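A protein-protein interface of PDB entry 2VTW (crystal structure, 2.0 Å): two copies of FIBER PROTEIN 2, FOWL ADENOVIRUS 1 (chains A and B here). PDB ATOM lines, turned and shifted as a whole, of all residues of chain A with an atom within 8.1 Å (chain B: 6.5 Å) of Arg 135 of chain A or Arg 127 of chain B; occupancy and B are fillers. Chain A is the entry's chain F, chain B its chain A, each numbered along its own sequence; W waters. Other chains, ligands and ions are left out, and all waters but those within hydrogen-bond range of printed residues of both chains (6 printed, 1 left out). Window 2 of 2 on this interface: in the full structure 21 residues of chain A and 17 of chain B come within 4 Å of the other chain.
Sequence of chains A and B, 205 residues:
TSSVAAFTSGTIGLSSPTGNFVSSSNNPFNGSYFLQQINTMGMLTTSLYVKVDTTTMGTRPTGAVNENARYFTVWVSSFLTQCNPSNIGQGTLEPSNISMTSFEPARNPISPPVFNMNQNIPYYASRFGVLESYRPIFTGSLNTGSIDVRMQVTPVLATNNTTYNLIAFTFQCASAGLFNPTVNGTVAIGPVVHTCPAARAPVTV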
ATOM      1  N   GLU A 132       5.098   9.304  12.526  1.00  0.00           N
ATOM      2  CA  GLU A 132       4.149   8.173  12.732  1.00  0.00           C
ATOM      3  C   GLU A 132       3.141   8.141  11.616  1.00  0.00           C
ATOM      4  O   GLU A 132       2.710   9.203  11.145  1.00  0.00           O
ATOM      5  CB  GLU A 132       3.381   8.334  14.058  1.00  0.00           C
ATOM      6  CG  GLU A 132       4.216   8.296  15.305  1.00  0.00           C
ATOM      7  CD  GLU A 132       4.631   6.896  15.724  1.00  0.00           C
ATOM      8  OE1 GLU A 132       4.448   5.915  14.983  1.00  0.00           O
ATOM      9  OE2 GLU A 132       5.168   6.769  16.824  1.00  0.00           O
ATOM     10  N   SER A 133       2.763   6.938  11.197  1.00  0.00           N
ATOM     11  CA  SER A 133       1.885   6.746  10.043  1.00  0.00           C
ATOM     12  C   SER A 133       0.451   6.404  10.456  1.00  0.00           C
ATOM     13  O   SER A 133       0.224   5.508  11.267  1.00  0.00           O
ATOM     14  CB  SER A 133       2.440   5.662   9.133  1.00  0.00           C
ATOM     15  OG  SER A 133       3.760   6.005   8.727  1.00  0.00           O
ATOM     16  N   TYR A 134      -0.493   7.162   9.925  1.00  0.00           N
ATOM     17  CA  TYR A 134      -1.926   6.979  10.201  1.00  0.00           C
ATOM     18  C   TYR A 134      -2.661   6.859   8.910  1.00  0.00           C
ATOM     19  O   TYR A 134      -2.241   7.447   7.903  1.00  0.00           O
ATOM     20  CB  TYR A 134      -2.498   8.188  10.966  1.00  0.00           C
ATOM     21  CG  TYR A 134      -1.840   8.340  12.265  1.00  0.00           C
ATOM     22  CD1 TYR A 134      -2.348   7.721  13.399  1.00  0.00           C
ATOM     23  CD2 TYR A 134      -0.647   9.039  12.361  1.00  0.00           C
ATOM     24  CE1 TYR A 134      -1.692   7.822  14.585  1.00  0.00           C
ATOM     25  CE2 TYR A 134       0.006   9.124  13.529  1.00  0.00           C
ATOM     26  CZ  TYR A 134      -0.502   8.501  14.622  1.00  0.00           C
ATOM     27  OH  TYR A 134       0.173   8.624  15.785  1.00  0.00           O
ATOM     28  N   ARG A 135      -3.761   6.114   8.926  1.00  0.00           N
ATOM     29  CA  ARG A 135      -4.762   6.238   7.889  1.00  0.00           C
ATOM     30  C   ARG A 135      -6.012   6.888   8.518  1.00  0.00           C
ATOM     31  O   ARG A 135      -6.559   6.364   9.506  1.00  0.00           O
ATOM     32  CB  ARG A 135      -5.092   4.862   7.278  1.00  0.00           C
ATOM     33  CG  ARG A 135      -6.171   4.932   6.219  1.00  0.00           C
ATOM     34  CD  ARG A 135      -6.682   3.558   5.788  1.00  0.00           C
ATOM     35  NE  ARG A 135      -5.736   2.844   4.911  1.00  0.00           N
ATOM     36  CZ  ARG A 135      -5.168   1.662   5.172  1.00  0.00           C
ATOM     37  NH1 ARG A 135      -5.429   0.979   6.286  1.00  0.00           N
ATOM     38  NH2 ARG A 135      -4.339   1.128   4.269  1.00  0.00           N
ATOM     39  N   PRO A 136      -6.461   8.025   7.967  1.00  0.00           N
ATOM     40  CA  PRO A 136      -7.677   8.720   8.427  1.00  0.00           C
ATOM     41  C   PRO A 136      -8.960   8.201   7.761  1.00  0.00           C
ATOM     42  O   PRO A 136      -8.877   7.395   6.857  1.00  0.00           O
ATOM     43  CB  PRO A 136      -7.436  10.145   7.953  1.00  0.00           C
ATOM     44  CG  PRO A 136      -6.761   9.962   6.653  1.00  0.00           C
ATOM     45  CD  PRO A 136      -5.857   8.736   6.824  1.00  0.00           C
ATOM     46  N   ILE A 137     -10.118   8.692   8.204  1.00  0.00           N
ATOM     47  CA  ILE A 137     -11.439   8.393   7.606  1.00  0.00           C
ATOM     48  C   ILE A 137     -11.982   9.593   6.817  1.00  0.00           C
ATOM     49  O   ILE A 137     -11.976  10.701   7.317  1.00  0.00           O
ATOM     50  CB  ILE A 137     -12.487   8.077   8.718  1.00  0.00           C
ATOM     51  CG1 ILE A 137     -12.168   6.769   9.448  1.00  0.00           C
ATOM     52  CG2 ILE A 137     -13.916   7.940   8.103  1.00  0.00           C
ATOM     53  CD1 ILE A 137     -13.167   5.643   9.141  1.00  0.00           C
ATOM     54  N   PHE A 138     -12.487   9.352   5.608  1.00  0.00           N
ATOM     55  CA  PHE A 138     -13.101  10.385   4.745  1.00  0.00           C
ATOM     56  C   PHE A 138     -14.582  10.261   4.596  1.00  0.00           C
ATOM     57  O   PHE A 138     -15.157   9.182   4.760  1.00  0.00           O
ATOM     58  CB  PHE A 138     -12.555  10.338   3.320  1.00  0.00           C
ATOM     59  CG  PHE A 138     -11.094  10.232   3.269  1.00  0.00           C
ATOM     60  CD1 PHE A 138     -10.328  11.225   3.808  1.00  0.00           C
ATOM     61  CD2 PHE A 138     -10.480   9.117   2.727  1.00  0.00           C
ATOM     62  CE1 PHE A 138      -8.970  11.115   3.818  1.00  0.00           C
ATOM     63  CE2 PHE A 138      -9.122   9.000   2.730  1.00  0.00           C
ATOM     64  CZ  PHE A 138      -8.370   9.985   3.268  1.00  0.00           C
ATOM     65  N   THR A 144      -7.262  12.227   0.967  1.00  0.00           N
ATOM     66  CA  THR A 144      -5.944  12.750   1.283  1.00  0.00           C
ATOM     67  C   THR A 144      -4.936  11.626   1.213  1.00  0.00           C
ATOM     68  O   THR A 144      -3.731  11.864   1.335  1.00  0.00           O
ATOM     69  CB  THR A 144      -5.896  13.305   2.741  1.00  0.00           C
ATOM     70  OG1 THR A 144      -6.246  12.273   3.669  1.00  0.00           O
ATOM     71  CG2 THR A 144      -6.839  14.500   2.929  1.00  0.00           C
ATOM     72  N   GLY A 145      -5.442  10.408   1.030  1.00  0.00           N
ATOM     73  CA  GLY A 145      -4.675   9.197   1.277  1.00  0.00           C
ATOM     74  C   GLY A 145      -4.285   9.087   2.745  1.00  0.00           C
ATOM     75  O   GLY A 145      -4.823   9.789   3.597  1.00  0.00           O
ATOM     76  N   SER A 146      -3.343   8.196   3.029  1.00  0.00           N
ATOM     77  CA  SER A 146      -2.688   8.169   4.314  1.00  0.00           C
ATOM     78  C   SER A 146      -1.966   9.478   4.700  1.00  0.00           C
ATOM     79  O   SER A 146      -1.572  10.294   3.841  1.00  0.00           O
ATOM     80  CB  SER A 146      -1.707   7.006   4.388  1.00  0.00           C
ATOM     81  OG  SER A 146      -2.428   5.829   4.692  1.00  0.00           O
ATOM     82  N   ILE A 147      -1.779   9.641   6.007  1.00  0.00           N
ATOM     83  CA  ILE A 147      -1.203  10.860   6.569  1.00  0.00           C
ATOM     84  C   ILE A 147      -0.104  10.510   7.567  1.00  0.00           C
ATOM     85  O   ILE A 147      -0.362   9.779   8.529  1.00  0.00           O
ATOM     86  CB  ILE A 147      -2.285  11.713   7.294  1.00  0.00           C
ATOM     87  CG1 ILE A 147      -3.379  12.155   6.299  1.00  0.00           C
ATOM     88  CG2 ILE A 147      -1.625  12.942   7.995  1.00  0.00           C
ATOM     89  CD1 ILE A 147      -4.532  12.909   6.928  1.00  0.00           C
ATOM     90  N   ASP A 148       1.114  11.001   7.335  1.00  0.00           N
ATOM     91  CA  ASP A 148       2.164  10.843   8.338  1.00  0.00           C
ATOM     92  C   ASP A 148       2.177  12.104   9.209  1.00  0.00           C
ATOM     93  O   ASP A 148       1.891  13.204   8.730  1.00  0.00           O
ATOM     94  CB  ASP A 148       3.541  10.657   7.722  1.00  0.00           C
ATOM     95  CG  ASP A 148       3.722   9.297   7.025  1.00  0.00           C
ATOM     96  OD1 ASP A 148       3.032   8.294   7.353  1.00  0.00           O
ATOM     97  OD2 ASP A 148       4.599   9.243   6.139  1.00  0.00           O
ATOM     98  N   VAL A 187     -12.281  14.926   6.735  1.00  0.00           N
ATOM     99  CA  VAL A 187     -11.212  13.969   7.072  1.00  0.00           C
ATOM    100  C   VAL A 187     -11.007  14.049   8.562  1.00  0.00           C
ATOM    101  O   VAL A 187     -10.943  15.160   9.151  1.00  0.00           O
ATOM    102  CB  VAL A 187      -9.879  14.281   6.348  1.00  0.00           C
ATOM    103  CG1 VAL A 187      -9.405  15.666   6.704  1.00  0.00           C
ATOM    104  CG2 VAL A 187      -8.798  13.215   6.646  1.00  0.00           C
ATOM    105  N   ALA A 188     -10.945  12.870   9.179  1.00  0.00           N
ATOM    106  CA  ALA A 188     -10.769  12.742  10.602  1.00  0.00           C
ATOM    107  C   ALA A 188      -9.604  11.786  10.851  1.00  0.00           C
ATOM    108  O   ALA A 188      -9.538  10.735  10.250  1.00  0.00           O
ATOM    109  CB  ALA A 188     -12.070  12.241  11.238  1.00  0.00           C
ATOM    110  N   ILE A 189      -8.687  12.169  11.727  1.00  0.00           N
ATOM    111  CA  ILE A 189      -7.449  11.421  12.004  1.00  0.00           C
ATOM    112  C   ILE A 189      -7.254  11.286  13.501  1.00  0.00           C
ATOM    113  O   ILE A 189      -7.515  12.205  14.276  1.00  0.00           O
ATOM    114  CB  ILE A 189      -6.184  12.094  11.343  1.00  0.00           C
ATOM    115  CG1 ILE A 189      -4.906  11.303  11.646  1.00  0.00           C
ATOM    116  CG2 ILE A 189      -6.018  13.531  11.794  1.00  0.00           C
ATOM    117  CD1 ILE A 189      -3.800  11.484  10.621  1.00  0.00           C
ATOM    118  N   GLY A 190      -6.831  10.092  13.894  1.00  0.00           N
ATOM    119  CA  GLY A 190      -6.348   9.852  15.222  1.00  0.00           C
ATOM    120  C   GLY A 190      -6.810   8.501  15.735  1.00  0.00           C
ATOM    121  O   GLY A 190      -7.355   7.681  14.970  1.00  0.00           O
ATOM    122  N   PRO A 191      -6.547   8.238  17.007  1.00  0.00           N
ATOM    123  CA  PRO A 191      -5.819   9.124  17.923  1.00  0.00           C
ATOM    124  C   PRO A 191      -4.319   9.179  17.581  1.00  0.00           C
ATOM    125  O   PRO A 191      -3.688   8.130  17.402  1.00  0.00           O
ATOM    126  CB  PRO A 191      -6.036   8.457  19.287  1.00  0.00           C
ATOM    127  CG  PRO A 191      -6.151   7.029  18.994  1.00  0.00           C
ATOM    128  CD  PRO A 191      -6.938   6.979  17.669  1.00  0.00           C
ATOM    129  N   TYR B  71      -2.740 -11.211   6.329  1.00  0.00           N
ATOM    130  CA  TYR B  71      -3.227 -10.435   7.493  1.00  0.00           C
ATOM    131  C   TYR B  71      -3.948 -11.310   8.485  1.00  0.00           C
ATOM    132  O   TYR B  71      -4.537 -12.309   8.119  1.00  0.00           O
ATOM    133  CB  TYR B  71      -4.176  -9.318   7.080  1.00  0.00           C
ATOM    134  CG  TYR B  71      -3.607  -8.213   6.230  1.00  0.00           C
ATOM    135  CD1 TYR B  71      -2.334  -8.292   5.635  1.00  0.00           C
ATOM    136  CD2 TYR B  71      -4.362  -7.096   5.972  1.00  0.00           C
ATOM    137  CE1 TYR B  71      -1.855  -7.260   4.845  1.00  0.00           C
ATOM    138  CE2 TYR B  71      -3.900  -6.090   5.167  1.00  0.00           C
ATOM    139  CZ  TYR B  71      -2.649  -6.164   4.626  1.00  0.00           C
ATOM    140  OH  TYR B  71      -2.220  -5.127   3.840  1.00  0.00           O
ATOM    141  N   ILE B 110     -13.610   9.113  15.226  1.00  0.00           N
ATOM    142  CA  ILE B 110     -13.479   9.098  13.781  1.00  0.00           C
ATOM    143  C   ILE B 110     -14.491   8.123  13.161  1.00  0.00           C
ATOM    144  O   ILE B 110     -14.698   8.145  11.957  1.00  0.00           O
ATOM    145  CB  ILE B 110     -12.011   8.828  13.311  1.00  0.00           C
ATOM    146  CG1 ILE B 110     -11.659   7.350  13.382  1.00  0.00           C
ATOM    147  CG2 ILE B 110     -11.005   9.696  14.126  1.00  0.00           C
ATOM    148  CD1 ILE B 110     -10.314   7.000  12.748  1.00  0.00           C
ATOM    149  N   TYR B 124     -12.361  -9.121  10.758  1.00  0.00           N
ATOM    150  CA  TYR B 124     -12.449  -7.680  10.606  1.00  0.00           C
ATOM    151  C   TYR B 124     -11.034  -7.100  10.363  1.00  0.00           C
ATOM    152  O   TYR B 124     -10.118  -7.370  11.142  1.00  0.00           O
ATOM    153  CB  TYR B 124     -13.059  -7.080  11.869  1.00  0.00           C
ATOM    154  CG  TYR B 124     -13.222  -5.574  11.801  1.00  0.00           C
ATOM    155  CD1 TYR B 124     -14.313  -5.006  11.152  1.00  0.00           C
ATOM    156  CD2 TYR B 124     -12.293  -4.721  12.386  1.00  0.00           C
ATOM    157  CE1 TYR B 124     -14.471  -3.643  11.078  1.00  0.00           C
ATOM    158  CE2 TYR B 124     -12.454  -3.341  12.314  1.00  0.00           C
ATOM    159  CZ  TYR B 124     -13.539  -2.821  11.656  1.00  0.00           C
ATOM    160  OH  TYR B 124     -13.730  -1.474  11.573  1.00  0.00           O
ATOM    161  N   ALA B 125     -10.885  -6.314   9.292  1.00  0.00           N
ATOM    162  CA  ALA B 125      -9.633  -5.599   8.957  1.00  0.00           C
ATOM    163  C   ALA B 125      -9.564  -4.252   9.679  1.00  0.00           C
ATOM    164  O   ALA B 125     -10.269  -3.315   9.307  1.00  0.00           O
ATOM    165  CB  ALA B 125      -9.540  -5.364   7.449  1.00  0.00           C
ATOM    166  N   SER B 126      -8.734  -4.184  10.718  1.00  0.00           N
ATOM    167  CA  SER B 126      -8.328  -2.914  11.345  1.00  0.00           C
ATOM    168  C   SER B 126      -7.686  -2.022  10.285  1.00  0.00           C
ATOM    169  O   SER B 126      -6.717  -2.422   9.648  1.00  0.00           O
ATOM    170  CB  SER B 126      -7.357  -3.213  12.470  1.00  0.00           C
ATOM    171  OG  SER B 126      -7.089  -2.088  13.268  1.00  0.00           O
ATOM    172  N   ARG B 127      -8.229  -0.824  10.072  1.00  0.00           N
ATOM    173  CA  ARG B 127      -7.731   0.057   8.994  1.00  0.00           C
ATOM    174  C   ARG B 127      -7.418   1.534   9.343  1.00  0.00           C
ATOM    175  O   ARG B 127      -6.676   2.189   8.608  1.00  0.00           O
ATOM    176  CB  ARG B 127      -8.721   0.020   7.844  1.00  0.00           C
ATOM    177  CG  ARG B 127      -8.648  -1.285   7.051  1.00  0.00           C
ATOM    178  CD  ARG B 127      -9.511  -1.283   5.804  1.00  0.00           C
ATOM    179  NE  ARG B 127      -9.269  -0.082   5.006  1.00  0.00           N
ATOM    180  CZ  ARG B 127      -8.263   0.100   4.155  1.00  0.00           C
ATOM    181  NH1 ARG B 127      -7.354  -0.854   3.921  1.00  0.00           N
ATOM    182  NH2 ARG B 127      -8.179   1.264   3.522  1.00  0.00           N
ATOM    183  N   PHE B 128      -7.987   2.063  10.432  1.00  0.00           N
ATOM    184  CA  PHE B 128      -7.984   3.513  10.669  1.00  0.00           C
ATOM    185  C   PHE B 128      -7.397   3.792  12.039  1.00  0.00           C
ATOM    186  O   PHE B 128      -8.018   3.526  13.070  1.00  0.00           O
ATOM    187  CB  PHE B 128      -9.404   4.107  10.530  1.00  0.00           C
ATOM    188  CG  PHE B 128     -10.069   3.755   9.232  1.00  0.00           C
ATOM    189  CD1 PHE B 128      -9.696   4.382   8.058  1.00  0.00           C
ATOM    190  CD2 PHE B 128     -11.017   2.737   9.173  1.00  0.00           C
ATOM    191  CE1 PHE B 128     -10.296   4.023   6.831  1.00  0.00           C
ATOM    192  CE2 PHE B 128     -11.610   2.372   7.976  1.00  0.00           C
ATOM    193  CZ  PHE B 128     -11.256   3.020   6.798  1.00  0.00           C
ATOM    194  N   GLY B 129      -6.198   4.359  12.033  1.00  0.00           N
ATOM    195  CA  GLY B 129      -5.409   4.520  13.224  1.00  0.00           C
ATOM    196  C   GLY B 129      -3.936   4.374  12.854  1.00  0.00           C
ATOM    197  O   GLY B 129      -3.567   4.419  11.671  1.00  0.00           O
ATOM    198  N   VAL B 130      -3.095   4.237  13.866  1.00  0.00           N
ATOM    199  CA  VAL B 130      -1.664   4.207  13.665  1.00  0.00           C
ATOM    200  C   VAL B 130      -1.262   2.846  13.079  1.00  0.00           C
ATOM    201  O   VAL B 130      -1.861   1.826  13.419  1.00  0.00           O
ATOM    202  CB  VAL B 130      -0.895   4.462  14.991  1.00  0.00           C
ATOM    203  CG1 VAL B 130      -0.944   3.257  15.902  1.00  0.00           C
ATOM    204  CG2 VAL B 130       0.557   4.861  14.706  1.00  0.00           C
ATOM    205  N   LEU B 131      -0.236   2.860  12.231  1.00  0.00           N
ATOM    206  CA  LEU B 131       0.410   1.648  11.717  1.00  0.00           C
ATOM    207  C   LEU B 131       1.834   1.600  12.241  1.00  0.00           C
ATOM    208  O   LEU B 131       2.618   2.515  11.954  1.00  0.00           O
ATOM    209  CB  LEU B 131       0.434   1.669  10.182  1.00  0.00           C
ATOM    210  CG  LEU B 131       1.010   0.418   9.523  1.00  0.00           C
ATOM    211  CD1 LEU B 131       0.037  -0.773   9.657  1.00  0.00           C
ATOM    212  CD2 LEU B 131       1.404   0.697   8.078  1.00  0.00           C
ATOM    213  N   ARG B 150      -1.781  -2.489  12.313  1.00  0.00           N
ATOM    214  CA  ARG B 150      -2.781  -1.416  12.392  1.00  0.00           C
ATOM    215  C   ARG B 150      -3.610  -1.554  13.668  1.00  0.00           C
ATOM    216  O   ARG B 150      -4.095  -2.629  13.980  1.00  0.00           O
ATOM    217  CB  ARG B 150      -3.688  -1.439  11.177  1.00  0.00           C
ATOM    218  CG  ARG B 150      -4.675  -0.251  11.094  1.00  0.00           C
ATOM    219  CD  ARG B 150      -3.989   1.002  10.690  1.00  0.00           C
ATOM    220  NE  ARG B 150      -3.472   0.927   9.331  1.00  0.00           N
ATOM    221  CZ  ARG B 150      -2.844   1.911   8.701  1.00  0.00           C
ATOM    222  NH1 ARG B 150      -2.611   3.059   9.303  1.00  0.00           N
ATOM    223  NH2 ARG B 150      -2.447   1.738   7.444  1.00  0.00           N
ATOM    224  N   MET B 151      -3.766  -0.460  14.414  1.00  0.00           N
ATOM    225  CA  MET B 151      -4.483  -0.499  15.679  1.00  0.00           C
ATOM    226  C   MET B 151      -5.661   0.503  15.656  1.00  0.00           C
ATOM    227  O   MET B 151      -5.474   1.698  15.379  1.00  0.00           O
ATOM    228  CB  MET B 151      -3.529  -0.236  16.823  1.00  0.00           C
ATOM    229  CG  MET B 151      -2.294  -1.161  16.827  1.00  0.00           C
ATOM    230  SD  MET B 151      -0.961  -0.458  17.795  1.00  0.00           S
ATOM    231  CE  MET B 151       0.444  -1.267  17.064  1.00  0.00           C
ATOM    232  N   GLN B 152      -6.871  -0.015  15.918  1.00  0.00           N
ATOM    233  CA  GLN B 152      -8.096   0.729  15.713  1.00  0.00           C
ATOM    234  C   GLN B 152      -9.127   0.375  16.789  1.00  0.00           C
ATOM    235  O   GLN B 152      -9.624  -0.762  16.851  1.00  0.00           O
ATOM    236  CB  GLN B 152      -8.659   0.443  14.328  1.00  0.00           C
ATOM    237  CG  GLN B 152      -9.936   1.231  13.953  1.00  0.00           C
ATOM    238  CD  GLN B 152     -10.651   0.577  12.790  1.00  0.00           C
ATOM    239  OE1 GLN B 152     -10.213   0.664  11.644  1.00  0.00           O
ATOM    240  NE2 GLN B 152     -11.746  -0.117  13.084  1.00  0.00           N
ATOM    241  N   THR B 170      -4.647  -5.557  13.651  1.00  0.00           N
ATOM    242  CA  THR B 170      -4.470  -6.373  12.450  1.00  0.00           C
ATOM    243  C   THR B 170      -2.991  -6.431  12.083  1.00  0.00           C
ATOM    244  O   THR B 170      -2.356  -5.397  11.807  1.00  0.00           O
ATOM    245  CB  THR B 170      -5.357  -5.951  11.271  1.00  0.00           C
ATOM    246  OG1 THR B 170      -6.748  -6.016  11.642  1.00  0.00           O
ATOM    247  CG2 THR B 170      -5.139  -6.869  10.072  1.00  0.00           C
ATOM    248  N   GLN B 172      -0.102  -7.370   9.690  1.00  0.00           N
ATOM    249  CA  GLN B 172       0.021  -7.383   8.254  1.00  0.00           C
ATOM    250  C   GLN B 172       1.417  -7.890   7.861  1.00  0.00           C
ATOM    251  O   GLN B 172       2.398  -7.120   7.868  1.00  0.00           O
ATOM    252  CB  GLN B 172      -0.247  -5.988   7.713  1.00  0.00           C
ATOM    253  CG  GLN B 172      -1.515  -5.354   8.340  1.00  0.00           C
ATOM    254  CD  GLN B 172      -1.899  -4.028   7.743  1.00  0.00           C
ATOM    255  OE1 GLN B 172      -3.061  -3.613   7.833  1.00  0.00           O
ATOM    256  NE2 GLN B 172      -0.942  -3.349   7.106  1.00  0.00           N
HETATM  257  O   HOH W   1       3.963   4.736  12.607  1.00  0.00           O
HETATM  258  O   HOH W   2      -8.399   5.182  15.337  1.00  0.00           O
HETATM  259  O   HOH W   3      -0.969   4.427   7.090  1.00  0.00           O
HETATM  260  O   HOH W   4      -3.880   5.337  16.626  1.00  0.00           O
HETATM  261  O   HOH W   5      -6.571   7.828  12.122  1.00  0.00           O
HETATM  262  O   HOH W   6      -4.586  -1.316   7.623  1.00  0.00           O
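The backbone NH (N) of Arg 135 of chain A lies close to the guanidinium group (NH1) of Arg 150 of chain B, at 3.3 Å.
The backbone carbonyl oxygen of Arg 127 of chain B lies within hydrogen-bond range of the guanidinium group of Arg 135 of chain A.
The backbone carbonyl oxygen of Ser 133 of chain A lies within hydrogen-bond range of the backbone NH of Leu 131 of chain B.
The backbone carbonyl oxygen (O) of Gly 129 of chain B sits at hydrogen-bond distance from the backbone NH (N) of Arg 135 of chain A (3.2 Å).
The side-chain hydroxyl (OG) of Ser 126 of chain B lies within hydrogen-bond range of the backbone carbonyl oxygen (O) of Arg 150 of chain B, 3.1 Å away.
The side-chain carboxylate (OD1) of Asp 148 of chain A sits at hydrogen-bond distance from the side-chain hydroxyl (OG) of Ser 133 of chain A, 2.8 Å away.
The backbone carbonyl oxygen (O) of Arg 150 of chain B lies within hydrogen-bond range of the backbone NH (N) of Thr 170 of chain B (3.0 Å).
The backbone NH of Ile 147 of chain A sits at hydrogen-bond distance from the backbone carbonyl oxygen of Tyr 134 of chain A, 2.9 Å away.
The guanidinium group (NH1) of Arg 150 of chain B lies within hydrogen-bond range of the backbone carbonyl oxygen (O) of Gly 129 of chain B, at 2.9 Å.
N of Ile 137 of chain A is in hydrogen-bond range of O of Ala 188 of chain A.
Ser 133 of chain A touches Gly 129 of chain B (O to O, 3.96 Å).
CA of Val 130 of chain B touches O of Ser 133 of chain A, 3.3 Å away.
Tyr 134 of chain A touches Gly 129 of chain B (CA to O, 3.4 Å).
Val 130 of chain B touches Tyr 134 of chain A (CB to CE1, 3.5 Å).
CA of Phe 128 of chain B touches O of Arg 135 of chain A (3.4 Å).
Pro 136 of chain A touches Phe 128 of chain B (O to CD1, 3.3 Å).
Ile 110 of chain B touches Ile 137 of chain A.
Phe 128 of chain B touches Ile 137 of chain A (CD2 to CD1, 3.6 Å).
CB of Ala 188 of chain A touches CB of Ile 110 of chain B, at 3.99 Å.
Ile 110 of chain B touches Gly 190 of chain A (CD1 to O, 3.8 Å).
Of the printed residues of chain B, Arg 135 of chain A touches Arg 127 (2.9 Å), Phe 128 (3.4 Å), Gly 129 (3.2 Å) and Arg 150 (3.3 Å).
Of the printed residues of chain B, Pro 136 of chain A touches Phe 128.
Gly 145 of chain A touches none of the printed residues of chain B.
Of the printed residues of chain B, Gly 190 of chain A touches Ile 110.
Of the printed residues of chain A, Ile 110 of chain B touches Ile 137 (3.8 Å), Ala 188 (3.99 Å) and Gly 190 (3.8 Å).
No residue of chain A comes within 4 Å of Ser 126 of chain B.
Of the printed residues of chain A, Phe 128 of chain B touches Arg 135 (3.4 Å), Pro 136 (3.3 Å) and Ile 137 (3.6 Å).
Of the printed residues of chain A, Leu 131 of chain B touches Ser 133.
The nearest printed residue of chain A that does not touch Ile 110 of chain B is Ile 189 of chain A (4.1 Å).
Of the 17 printed residues of chain A, 7 touch a printed residue of chain B.
Printed residues of chain A that touch a printed residue of chain B: Ser 133, Tyr 134, Arg 135, Pro 136, Ile 137, Ala 188 and Gly 190.
Among the printed residues, 15 pairs touch across the chains.
Among the printed residues, no Asp or Glu carboxylate lies within 4 Å of a Lys or Arg side-chain nitrogen of the other chain.
No position is printed for both chains.
Water W1 lies within hydrogen-bond range of the backbone carbonyl oxygen (O) of Leu 131 of chain B (2.7 Å), the side-chain carboxylate (OE1) of Glu 132 of chain A (2.7 Å) and the backbone NH (N) of Ser 133 of chain A (2.9 Å).
Water W2 lies within hydrogen-bond range of O of Gly 190 of chain A (2.7 Å) and O of Phe 128 of chain B (2.8 Å).
Water W6 lies within hydrogen-bond range of OE1 of Gln 172 of chain B (2.8 Å), NH1 of Arg 135 of chain A (2.8 Å), NE of Arg 150 of chain B (3.0 Å) and O of Ser 126 of chain B (3.1 Å).
Water W5 lies within hydrogen-bond range of N of Gly 190 of chain A (2.9 Å), O of Arg 135 of chain A (3.0 Å) and N of Gly 129 of chain B (3.5 Å).
Water W4 lies within hydrogen-bond range of the backbone carbonyl oxygen (O) of Pro 191 of chain A (2.9 Å) and the backbone NH (N) of Val 130 of chain B (3.1 Å).
Water W3 lies within hydrogen-bond range of NH1 of Arg 150 of chain B (3.1 Å), OG of Ser 146 of chain A (3.1 Å) and O of Tyr 134 of chain A (3.4 Å).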
